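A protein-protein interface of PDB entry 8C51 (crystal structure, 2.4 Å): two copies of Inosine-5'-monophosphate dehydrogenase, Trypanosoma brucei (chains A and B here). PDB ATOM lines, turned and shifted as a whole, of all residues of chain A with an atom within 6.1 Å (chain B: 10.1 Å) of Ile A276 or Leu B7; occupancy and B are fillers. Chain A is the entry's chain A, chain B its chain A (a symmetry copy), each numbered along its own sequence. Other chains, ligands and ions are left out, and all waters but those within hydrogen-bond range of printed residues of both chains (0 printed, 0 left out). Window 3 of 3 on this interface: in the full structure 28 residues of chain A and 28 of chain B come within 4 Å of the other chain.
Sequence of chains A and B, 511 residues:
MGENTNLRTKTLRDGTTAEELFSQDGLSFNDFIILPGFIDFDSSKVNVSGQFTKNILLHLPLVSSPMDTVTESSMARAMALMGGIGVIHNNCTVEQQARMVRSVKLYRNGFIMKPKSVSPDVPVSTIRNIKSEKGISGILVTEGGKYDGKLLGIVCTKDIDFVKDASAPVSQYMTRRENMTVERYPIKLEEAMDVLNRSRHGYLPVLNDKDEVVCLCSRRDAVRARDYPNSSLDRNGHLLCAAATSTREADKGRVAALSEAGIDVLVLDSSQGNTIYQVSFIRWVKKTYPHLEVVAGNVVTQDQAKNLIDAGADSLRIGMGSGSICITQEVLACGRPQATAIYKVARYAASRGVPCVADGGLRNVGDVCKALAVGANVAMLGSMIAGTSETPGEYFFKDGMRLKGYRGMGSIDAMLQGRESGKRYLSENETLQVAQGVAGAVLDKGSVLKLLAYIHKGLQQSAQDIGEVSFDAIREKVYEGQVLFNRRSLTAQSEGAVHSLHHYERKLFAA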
ATOM      1  N   GLY A 273      -9.300   9.255  25.253  1.00  0.00           N
ATOM      2  CA  GLY A 273     -10.502   9.911  25.724  1.00  0.00           C
ATOM      3  C   GLY A 273     -10.410  11.397  25.964  1.00  0.00           C
ATOM      4  O   GLY A 273     -11.426  12.024  26.270  1.00  0.00           O
ATOM      5  N   ASN A 274      -9.222  11.988  25.843  1.00  0.00           N
ATOM      6  CA  ASN A 274      -9.056  13.427  26.036  1.00  0.00           C
ATOM      7  C   ASN A 274      -9.404  14.155  24.735  1.00  0.00           C
ATOM      8  O   ASN A 274      -8.551  14.692  24.027  1.00  0.00           O
ATOM      9  CB  ASN A 274      -7.641  13.745  26.491  1.00  0.00           C
ATOM     10  CG  ASN A 274      -7.473  15.194  26.908  1.00  0.00           C
ATOM     11  OD1 ASN A 274      -8.424  15.841  27.342  1.00  0.00           O
ATOM     12  ND2 ASN A 274      -6.255  15.707  26.786  1.00  0.00           N
ATOM     13  N   THR A 275     -10.700  14.160  24.428  1.00  0.00           N
ATOM     14  CA  THR A 275     -11.213  14.804  23.229  1.00  0.00           C
ATOM     15  C   THR A 275     -12.304  15.798  23.600  1.00  0.00           C
ATOM     16  O   THR A 275     -12.920  15.714  24.664  1.00  0.00           O
ATOM     17  CB  THR A 275     -11.787  13.787  22.231  1.00  0.00           C
ATOM     18  OG1 THR A 275     -12.986  13.216  22.773  1.00  0.00           O
ATOM     19  CG2 THR A 275     -10.781  12.679  21.941  1.00  0.00           C
ATOM     20  N   ILE A 276     -12.544  16.741  22.687  1.00  0.00           N
ATOM     21  CA  ILE A 276     -13.628  17.698  22.884  1.00  0.00           C
ATOM     22  C   ILE A 276     -14.974  16.991  22.829  1.00  0.00           C
ATOM     23  O   ILE A 276     -15.920  17.377  23.529  1.00  0.00           O
ATOM     24  CB  ILE A 276     -13.535  18.821  21.836  1.00  0.00           C
ATOM     25  CG1 ILE A 276     -14.524  19.942  22.157  1.00  0.00           C
ATOM     26  CG2 ILE A 276     -13.804  18.271  20.443  1.00  0.00           C
ATOM     27  CD1 ILE A 276     -14.266  20.619  23.488  1.00  0.00           C
ATOM     28  N   TYR A 277     -15.084  15.946  22.005  1.00  0.00           N
ATOM     29  CA  TYR A 277     -16.343  15.220  21.898  1.00  0.00           C
ATOM     30  C   TYR A 277     -16.670  14.514  23.204  1.00  0.00           C
ATOM     31  O   TYR A 277     -17.822  14.517  23.647  1.00  0.00           O
ATOM     32  CB  TYR A 277     -16.279  14.220  20.742  1.00  0.00           C
ATOM     33  CG  TYR A 277     -15.534  14.735  19.529  1.00  0.00           C
ATOM     34  CD1 TYR A 277     -16.142  15.602  18.633  1.00  0.00           C
ATOM     35  CD2 TYR A 277     -14.218  14.360  19.288  1.00  0.00           C
ATOM     36  CE1 TYR A 277     -15.462  16.081  17.526  1.00  0.00           C
ATOM     37  CE2 TYR A 277     -13.530  14.832  18.185  1.00  0.00           C
ATOM     38  CZ  TYR A 277     -14.158  15.692  17.307  1.00  0.00           C
ATOM     39  OH  TYR A 277     -13.480  16.167  16.206  1.00  0.00           O
ATOM     40  N   GLN A 278     -15.661  13.941  23.862  1.00  0.00           N
ATOM     41  CA  GLN A 278     -15.913  13.260  25.127  1.00  0.00           C
ATOM     42  C   GLN A 278     -16.198  14.255  26.247  1.00  0.00           C
ATOM     43  O   GLN A 278     -17.030  13.987  27.119  1.00  0.00           O
ATOM     44  CB  GLN A 278     -14.732  12.366  25.502  1.00  0.00           C
ATOM     45  CG  GLN A 278     -15.003  11.544  26.758  1.00  0.00           C
ATOM     46  CD  GLN A 278     -14.159  10.282  26.868  1.00  0.00           C
ATOM     47  OE1 GLN A 278     -13.709   9.925  27.959  1.00  0.00           O
ATOM     48  NE2 GLN A 278     -13.958   9.591  25.748  1.00  0.00           N
ATOM     49  N   VAL A 279     -15.513  15.399  26.252  1.00  0.00           N
ATOM     50  CA  VAL A 279     -15.801  16.424  27.254  1.00  0.00           C
ATOM     51  C   VAL A 279     -17.245  16.896  27.115  1.00  0.00           C
ATOM     52  O   VAL A 279     -17.998  16.969  28.100  1.00  0.00           O
ATOM     53  CB  VAL A 279     -14.806  17.592  27.124  1.00  0.00           C
ATOM     54  CG1 VAL A 279     -15.343  18.842  27.812  1.00  0.00           C
ATOM     55  CG2 VAL A 279     -13.449  17.196  27.697  1.00  0.00           C
ATOM     56  N   SER A 280     -17.654  17.217  25.885  1.00  0.00           N
ATOM     57  CA  SER A 280     -19.034  17.624  25.651  1.00  0.00           C
ATOM     58  C   SER A 280     -20.000  16.521  26.054  1.00  0.00           C
ATOM     59  O   SER A 280     -21.049  16.792  26.649  1.00  0.00           O
ATOM     60  CB  SER A 280     -19.231  17.994  24.181  1.00  0.00           C
ATOM     61  OG  SER A 280     -18.138  18.755  23.699  1.00  0.00           O
ATOM     62  N   PHE A 281     -19.665  15.269  25.736  1.00  0.00           N
ATOM     63  CA  PHE A 281     -20.550  14.162  26.068  1.00  0.00           C
ATOM     64  C   PHE A 281     -20.716  14.014  27.574  1.00  0.00           C
ATOM     65  O   PHE A 281     -21.826  13.775  28.059  1.00  0.00           O
ATOM     66  CB  PHE A 281     -20.014  12.869  25.461  1.00  0.00           C
ATOM     67  CG  PHE A 281     -21.085  11.883  25.117  1.00  0.00           C
ATOM     68  CD1 PHE A 281     -21.775  11.981  23.923  1.00  0.00           C
ATOM     69  CD2 PHE A 281     -21.410  10.864  25.992  1.00  0.00           C
ATOM     70  CE1 PHE A 281     -22.767  11.076  23.605  1.00  0.00           C
ATOM     71  CE2 PHE A 281     -22.400   9.957  25.682  1.00  0.00           C
ATOM     72  CZ  PHE A 281     -23.080  10.062  24.486  1.00  0.00           C
ATOM     73  N   ASN A 307      -8.736  17.370  32.241  1.00  0.00           N
ATOM     74  CA  ASN A 307      -9.823  17.781  31.360  1.00  0.00           C
ATOM     75  C   ASN A 307     -11.081  16.958  31.619  1.00  0.00           C
ATOM     76  O   ASN A 307     -12.182  17.507  31.755  1.00  0.00           O
ATOM     77  CB  ASN A 307      -9.382  17.654  29.901  1.00  0.00           C
ATOM     78  CG  ASN A 307      -8.531  18.825  29.442  1.00  0.00           C
ATOM     79  OD1 ASN A 307      -8.529  19.887  30.064  1.00  0.00           O
ATOM     80  ND2 ASN A 307      -7.799  18.633  28.349  1.00  0.00           N
ATOM     81  N   ASN B   4      -9.669  25.964  21.781  1.00  0.00           N
ATOM     82  CA  ASN B   4      -9.621  25.148  22.988  1.00  0.00           C
ATOM     83  C   ASN B   4      -8.231  25.158  23.602  1.00  0.00           C
ATOM     84  O   ASN B   4      -7.744  24.126  24.065  1.00  0.00           O
ATOM     85  CB  ASN B   4     -10.028  23.708  22.683  1.00  0.00           C
ATOM     86  CG  ASN B   4     -11.391  23.614  22.034  1.00  0.00           C
ATOM     87  OD1 ASN B   4     -12.327  24.314  22.423  1.00  0.00           O
ATOM     88  ND2 ASN B   4     -11.514  22.739  21.042  1.00  0.00           N
ATOM     89  N   THR B   5      -7.589  26.327  23.607  1.00  0.00           N
ATOM     90  CA  THR B   5      -6.228  26.406  24.125  1.00  0.00           C
ATOM     91  C   THR B   5      -6.179  26.051  25.604  1.00  0.00           C
ATOM     92  O   THR B   5      -5.172  25.512  26.078  1.00  0.00           O
ATOM     93  CB  THR B   5      -5.658  27.806  23.892  1.00  0.00           C
ATOM     94  OG1 THR B   5      -6.588  28.792  24.359  1.00  0.00           O
ATOM     95  CG2 THR B   5      -5.389  28.025  22.407  1.00  0.00           C
ATOM     96  N   ASN B   6      -7.249  26.339  26.348  1.00  0.00           N
ATOM     97  CA  ASN B   6      -7.285  25.950  27.754  1.00  0.00           C
ATOM     98  C   ASN B   6      -7.227  24.435  27.901  1.00  0.00           C
ATOM     99  O   ASN B   6      -6.573  23.919  28.815  1.00  0.00           O
ATOM    100  CB  ASN B   6      -8.544  26.506  28.423  1.00  0.00           C
ATOM    101  CG  ASN B   6      -8.236  27.250  29.710  1.00  0.00           C
ATOM    102  OD1 ASN B   6      -7.740  26.666  30.675  1.00  0.00           O
ATOM    103  ND2 ASN B   6      -8.529  28.547  29.729  1.00  0.00           N
ATOM    104  N   LEU B   7      -7.895  23.705  27.003  1.00  0.00           N
ATOM    105  CA  LEU B   7      -7.927  22.249  27.100  1.00  0.00           C
ATOM    106  C   LEU B   7      -6.697  21.596  26.481  1.00  0.00           C
ATOM    107  O   LEU B   7      -6.274  20.529  26.937  1.00  0.00           O
ATOM    108  CB  LEU B   7      -9.183  21.701  26.420  1.00  0.00           C
ATOM    109  CG  LEU B   7     -10.528  21.975  27.093  1.00  0.00           C
ATOM    110  CD1 LEU B   7     -11.655  21.805  26.089  1.00  0.00           C
ATOM    111  CD2 LEU B   7     -10.737  21.057  28.286  1.00  0.00           C
ATOM    112  N   ARG B   8      -6.110  22.213  25.453  1.00  0.00           N
ATOM    113  CA  ARG B   8      -4.962  21.611  24.788  1.00  0.00           C
ATOM    114  C   ARG B   8      -3.659  21.901  25.516  1.00  0.00           C
ATOM    115  O   ARG B   8      -2.723  21.096  25.447  1.00  0.00           O
ATOM    116  CB  ARG B   8      -4.860  22.118  23.350  1.00  0.00           C
ATOM    117  CG  ARG B   8      -3.463  22.001  22.749  1.00  0.00           C
ATOM    118  CD  ARG B   8      -3.497  21.996  21.229  1.00  0.00           C
ATOM    119  NE  ARG B   8      -4.265  20.868  20.714  1.00  0.00           N
ATOM    120  CZ  ARG B   8      -5.528  20.932  20.308  1.00  0.00           C
ATOM    121  NH1 ARG B   8      -6.197  22.074  20.296  1.00  0.00           N
ATOM    122  NH2 ARG B   8      -6.139  19.819  19.915  1.00  0.00           N
ATOM    123  N   THR B   9      -3.577  23.031  26.212  1.00  0.00           N
ATOM    124  CA  THR B   9      -2.327  23.460  26.821  1.00  0.00           C
ATOM    125  C   THR B   9      -2.085  22.677  28.105  1.00  0.00           C
ATOM    126  O   THR B   9      -2.898  22.727  29.035  1.00  0.00           O
ATOM    127  CB  THR B   9      -2.360  24.960  27.101  1.00  0.00           C
ATOM    128  OG1 THR B   9      -2.405  25.675  25.860  1.00  0.00           O
ATOM    129  CG2 THR B   9      -1.124  25.383  27.882  1.00  0.00           C
ATOM    130  N   LYS B  10      -0.968  21.955  28.152  1.00  0.00           N
ATOM    131  CA  LYS B  10      -0.596  21.193  29.335  1.00  0.00           C
ATOM    132  C   LYS B  10       0.052  22.126  30.349  1.00  0.00           C
ATOM    133  O   LYS B  10       1.050  22.786  30.041  1.00  0.00           O
ATOM    134  CB  LYS B  10       0.362  20.061  28.973  1.00  0.00           C
ATOM    135  CG  LYS B  10      -0.121  19.134  27.869  1.00  0.00           C
ATOM    136  CD  LYS B  10       0.865  17.988  27.666  1.00  0.00           C
ATOM    137  CE  LYS B  10       0.440  17.056  26.542  1.00  0.00           C
ATOM    138  NZ  LYS B  10      -0.017  17.791  25.328  1.00  0.00           N
ATOM    139  N   THR B  11      -0.515  22.189  31.548  1.00  0.00           N
ATOM    140  CA  THR B  11       0.094  22.897  32.666  1.00  0.00           C
ATOM    141  C   THR B  11       0.702  21.953  33.689  1.00  0.00           C
ATOM    142  O   THR B  11       1.802  22.208  34.180  1.00  0.00           O
ATOM    143  CB  THR B  11      -0.938  23.800  33.355  1.00  0.00           C
ATOM    144  OG1 THR B  11      -2.080  23.030  33.747  1.00  0.00           O
ATOM    145  CG2 THR B  11      -1.381  24.913  32.415  1.00  0.00           C
ATOM    146  N   LEU B  12       0.011  20.858  34.013  1.00  0.00           N
ATOM    147  CA  LEU B  12       0.611  19.832  34.859  1.00  0.00           C
ATOM    148  C   LEU B  12       1.865  19.257  34.211  1.00  0.00           C
ATOM    149  O   LEU B  12       2.855  18.975  34.896  1.00  0.00           O
ATOM    150  CB  LEU B  12      -0.405  18.725  35.132  1.00  0.00           C
ATOM    151  CG  LEU B  12      -1.594  19.116  36.010  1.00  0.00           C
ATOM    152  CD1 LEU B  12      -2.729  18.122  35.854  1.00  0.00           C
ATOM    153  CD2 LEU B  12      -1.165  19.217  37.463  1.00  0.00           C
ATOM    154  N   PRO B  36      -0.133  10.971  24.823  1.00  0.00           N
ATOM    155  CA  PRO B  36      -1.232  11.621  24.103  1.00  0.00           C
ATOM    156  C   PRO B  36      -1.522  13.017  24.633  1.00  0.00           C
ATOM    157  O   PRO B  36      -1.137  13.394  25.742  1.00  0.00           O
ATOM    158  CB  PRO B  36      -2.419  10.682  24.348  1.00  0.00           C
ATOM    159  CG  PRO B  36      -2.113  10.026  25.642  1.00  0.00           C
ATOM    160  CD  PRO B  36      -0.616   9.902  25.716  1.00  0.00           C
ATOM    161  N   GLY B  37      -2.211  13.790  23.795  1.00  0.00           N
ATOM    162  CA  GLY B  37      -2.593  15.144  24.132  1.00  0.00           C
ATOM    163  C   GLY B  37      -4.095  15.335  24.094  1.00  0.00           C
ATOM    164  O   GLY B  37      -4.840  14.551  24.690  1.00  0.00           O
ATOM    165  N   PHE B  38      -4.551  16.365  23.384  1.00  0.00           N
ATOM    166  CA  PHE B  38      -5.963  16.716  23.311  1.00  0.00           C
ATOM    167  C   PHE B  38      -6.415  16.716  21.857  1.00  0.00           C
ATOM    168  O   PHE B  38      -5.740  17.285  20.994  1.00  0.00           O
ATOM    169  CB  PHE B  38      -6.213  18.084  23.945  1.00  0.00           C
ATOM    170  CG  PHE B  38      -7.632  18.542  23.836  1.00  0.00           C
ATOM    171  CD1 PHE B  38      -8.594  18.060  24.705  1.00  0.00           C
ATOM    172  CD2 PHE B  38      -8.009  19.440  22.855  1.00  0.00           C
ATOM    173  CE1 PHE B  38      -9.903  18.472  24.605  1.00  0.00           C
ATOM    174  CE2 PHE B  38      -9.316  19.857  22.749  1.00  0.00           C
ATOM    175  CZ  PHE B  38     -10.267  19.371  23.625  1.00  0.00           C
ATOM    176  N   ILE B  39      -7.564  16.098  21.593  1.00  0.00           N
ATOM    177  CA  ILE B  39      -8.079  15.915  20.240  1.00  0.00           C
ATOM    178  C   ILE B  39      -9.333  16.764  20.076  1.00  0.00           C
ATOM    179  O   ILE B  39     -10.252  16.689  20.900  1.00  0.00           O
ATOM    180  CB  ILE B  39      -8.387  14.435  19.953  1.00  0.00           C
ATOM    181  CG1 ILE B  39      -7.113  13.589  20.007  1.00  0.00           C
ATOM    182  CG2 ILE B  39      -9.050  14.287  18.597  1.00  0.00           C
ATOM    183  CD1 ILE B  39      -7.379  12.101  20.173  1.00  0.00           C
ATOM    184  N   ASP B  40      -9.376  17.566  19.012  1.00  0.00           N
ATOM    185  CA  ASP B  40     -10.587  18.305  18.670  1.00  0.00           C
ATOM    186  C   ASP B  40     -10.709  18.421  17.158  1.00  0.00           C
ATOM    187  O   ASP B  40     -11.204  19.422  16.630  1.00  0.00           O
ATOM    188  CB  ASP B  40     -10.603  19.691  19.319  1.00  0.00           C
ATOM    189  CG  ASP B  40      -9.469  20.574  18.838  1.00  0.00           C
ATOM    190  OD1 ASP B  40      -9.415  21.750  19.253  1.00  0.00           O
ATOM    191  OD2 ASP B  40      -8.629  20.090  18.054  1.00  0.00           O
ATOM    192  N   PHE B  41     -10.283  17.383  16.448  1.00  0.00           N
ATOM    193  CA  PHE B  41     -10.293  17.396  14.994  1.00  0.00           C
ATOM    194  C   PHE B  41     -10.258  15.954  14.512  1.00  0.00           C
ATOM    195  O   PHE B  41      -9.813  15.055  15.229  1.00  0.00           O
ATOM    196  CB  PHE B  41      -9.096  18.170  14.437  1.00  0.00           C
ATOM    197  CG  PHE B  41      -7.773  17.622  14.884  1.00  0.00           C
ATOM    198  CD1 PHE B  41      -7.205  18.033  16.077  1.00  0.00           C
ATOM    199  CD2 PHE B  41      -7.110  16.673  14.124  1.00  0.00           C
ATOM    200  CE1 PHE B  41      -5.995  17.521  16.496  1.00  0.00           C
ATOM    201  CE2 PHE B  41      -5.900  16.156  14.537  1.00  0.00           C
ATOM    202  CZ  PHE B  41      -5.341  16.580  15.725  1.00  0.00           C
ATOM    203  N   ASP B  42     -10.707  15.749  13.280  1.00  0.00           N
ATOM    204  CA  ASP B  42     -10.632  14.430  12.668  1.00  0.00           C
ATOM    205  C   ASP B  42      -9.267  14.246  12.012  1.00  0.00           C
ATOM    206  O   ASP B  42      -8.663  15.197  11.507  1.00  0.00           O
ATOM    207  CB  ASP B  42     -11.764  14.243  11.656  1.00  0.00           C
ATOM    208  CG  ASP B  42     -11.447  13.197  10.608  1.00  0.00           C
ATOM    209  OD1 ASP B  42     -11.475  11.992  10.933  1.00  0.00           O
ATOM    210  OD2 ASP B  42     -11.182  13.583   9.452  1.00  0.00           O
ATOM    211  N   GLN B 464      -3.069  12.742  15.366  1.00  0.00           N
ATOM    212  CA  GLN B 464      -4.327  12.984  16.064  1.00  0.00           C
ATOM    213  C   GLN B 464      -4.226  12.538  17.515  1.00  0.00           C
ATOM    214  O   GLN B 464      -4.512  13.312  18.436  1.00  0.00           O
ATOM    215  CB  GLN B 464      -5.481  12.268  15.364  1.00  0.00           C
ATOM    216  CG  GLN B 464      -6.841  12.584  15.976  1.00  0.00           C
ATOM    217  CD  GLN B 464      -7.942  11.679  15.463  1.00  0.00           C
ATOM    218  OE1 GLN B 464      -7.679  10.596  14.941  1.00  0.00           O
ATOM    219  NE2 GLN B 464      -9.186  12.120  15.611  1.00  0.00           N
ATOM    220  N   ILE B 466      -1.740  12.268  19.310  1.00  0.00           N
ATOM    221  CA  ILE B 466      -0.844  13.173  20.017  1.00  0.00           C
ATOM    222  C   ILE B 466      -1.508  14.513  20.306  1.00  0.00           C
ATOM    223  O   ILE B 466      -1.098  15.214  21.240  1.00  0.00           O
ATOM    224  CB  ILE B 466       0.452  13.377  19.213  1.00  0.00           C
ATOM    225  CG1 ILE B 466       1.274  12.087  19.203  1.00  0.00           C
ATOM    226  CG2 ILE B 466       1.275  14.520  19.798  1.00  0.00           C
ATOM    227  CD1 ILE B 466       2.321  12.047  18.119  1.00  0.00           C
ATOM    228  N   GLY B 467      -2.515  14.892  19.530  1.00  0.00           N
ATOM    229  CA  GLY B 467      -3.272  16.095  19.794  1.00  0.00           C
ATOM    230  C   GLY B 467      -2.841  17.322  19.027  1.00  0.00           C
ATOM    231  O   GLY B 467      -3.125  18.438  19.477  1.00  0.00           O
ATOM    232  N   GLU B 468      -2.171  17.160  17.891  1.00  0.00           N
ATOM    233  CA  GLU B 468      -1.749  18.281  17.067  1.00  0.00           C
ATOM    234  C   GLU B 468      -2.121  18.006  15.616  1.00  0.00           C
ATOM    235  O   GLU B 468      -2.082  16.862  15.151  1.00  0.00           O
ATOM    236  CB  GLU B 468      -0.245  18.532  17.201  1.00  0.00           C
ATOM    237  CG  GLU B 468       0.193  18.895  18.614  1.00  0.00           C
ATOM    238  CD  GLU B 468      -0.394  20.211  19.090  1.00  0.00           C
ATOM    239  OE1 GLU B 468      -0.774  21.039  18.233  1.00  0.00           O
ATOM    240  OE2 GLU B 468      -0.472  20.419  20.320  1.00  0.00           O
ATOM    241  N   GLN B 482       5.665  20.921  25.201  1.00  0.00           N
ATOM    242  CA  GLN B 482       4.234  20.662  25.300  1.00  0.00           C
ATOM    243  C   GLN B 482       3.824  19.310  24.731  1.00  0.00           C
ATOM    244  O   GLN B 482       2.735  18.823  25.057  1.00  0.00           O
ATOM    245  CB  GLN B 482       3.446  21.767  24.587  1.00  0.00           C
ATOM    246  CG  GLN B 482       3.301  23.039  25.409  1.00  0.00           C
ATOM    247  CD  GLN B 482       2.278  22.898  26.523  1.00  0.00           C
ATOM    248  OE1 GLN B 482       1.146  22.475  26.293  1.00  0.00           O
ATOM    249  NE2 GLN B 482       2.676  23.251  27.739  1.00  0.00           N
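The side-chain hydroxyl (OH) of Tyr A277 is in hydrogen-bond range of the backbone NH (N) of Phe B41, 3.4 Å away.
The backbone carbonyl oxygen (O) of Ile B39 is in hydrogen-bond range of the backbone NH (N) of Ile A276, 2.9 Å away.
The side-chain amide nitrogen of Asn A307 sits at hydrogen-bond distance from the backbone carbonyl oxygen of Leu B7 (2.8 Å).
ND2 of Asn A274 sits at hydrogen-bond distance from O of Gly B37, at 2.8 Å.
The backbone carbonyl oxygen of Asn A274 sits at hydrogen-bond distance from the backbone NH of Ile B39.
Phe B38 touches Asn A274.
Phe B38 touches Thr A275.
Thr A275 touches Ile B39.
CD1 of Ile A276 touches CD1 of Leu B7, at 3.9 Å.
N of Ile A276 touches CZ of Phe B38 (3.6 Å).
Asp B40 touches Ile A276 (CA to CG2, 3.7 Å).
Asp B40 touches Tyr A277.
Asn A307 touches Phe B38 (ND2 to CD1, 3.8 Å).
Of the 21 printed residues of chain B, 6 touch a printed residue of chain A.
Printed residues of chain B that touch a printed residue of chain A: Leu B7, Gly B37, Phe B38, Ile B39, Asp B40 and Phe B41.
Hydrophobic or aromatic side chains of chain B within 4 Å of the printed part of chain A: Leu B7, Phe B38 and Ile B39.
Of the 10 printed residues of chain A, 5 touch a printed residue of chain B.
Among the printed residues, 13 pairs touch across the chains.
Thr A275 touches just these residues of chain B: Phe B38 and Ile B39.
Of chain B, only Leu B7 and Phe B38 come within 4 Å of Asn A307.
Of chain A, only Ile A276 and Asn A307 come within 4 Å of Leu B7.
Printed residues of chain A within 4 Å of Gly B37: Asn A274 (2.8 Å).
Printed residues of chain A within 4 Å of Phe B38: Asn A274 (3.4 Å), Thr A275 (3.7 Å), Ile A276 (3.6 Å) and Asn A307 (3.8 Å).
Printed residues of chain A within 4 Å of Ile B39: Asn A274 (3.0 Å), Thr A275 (3.1 Å) and Ile A276 (2.9 Å).
Gly B467 touches none of the printed residues of chain A.
The nearest residue of chain A that does not touch Leu B7 is Val A279 (4.8 Å).
N of Gln A278 lies within hydrogen-bond range of OG1 of Thr A275 (3.0 Å).
The guanidinium group (NH2) of Arg B8 is in salt-bridge range of the side-chain carboxylate (OD2) of Asp B40, at 3.1 Å.
NH2 of Arg B8 sits at hydrogen-bond distance from O of Phe B38.
The side-chain amide nitrogen (ND2) of Asn B4 sits at hydrogen-bond distance from the side-chain carboxylate (OD1) of Asp B40.
The side-chain hydroxyl (OG) of Ser A280 sits at hydrogen-bond distance from the backbone carbonyl oxygen (O) of Ile A276.
The side-chain amide oxygen (OD1) of Asn A274 sits at hydrogen-bond distance from the side-chain amide nitrogen (ND2) of Asn A307 (3.0 Å).
No position is printed for both chains.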
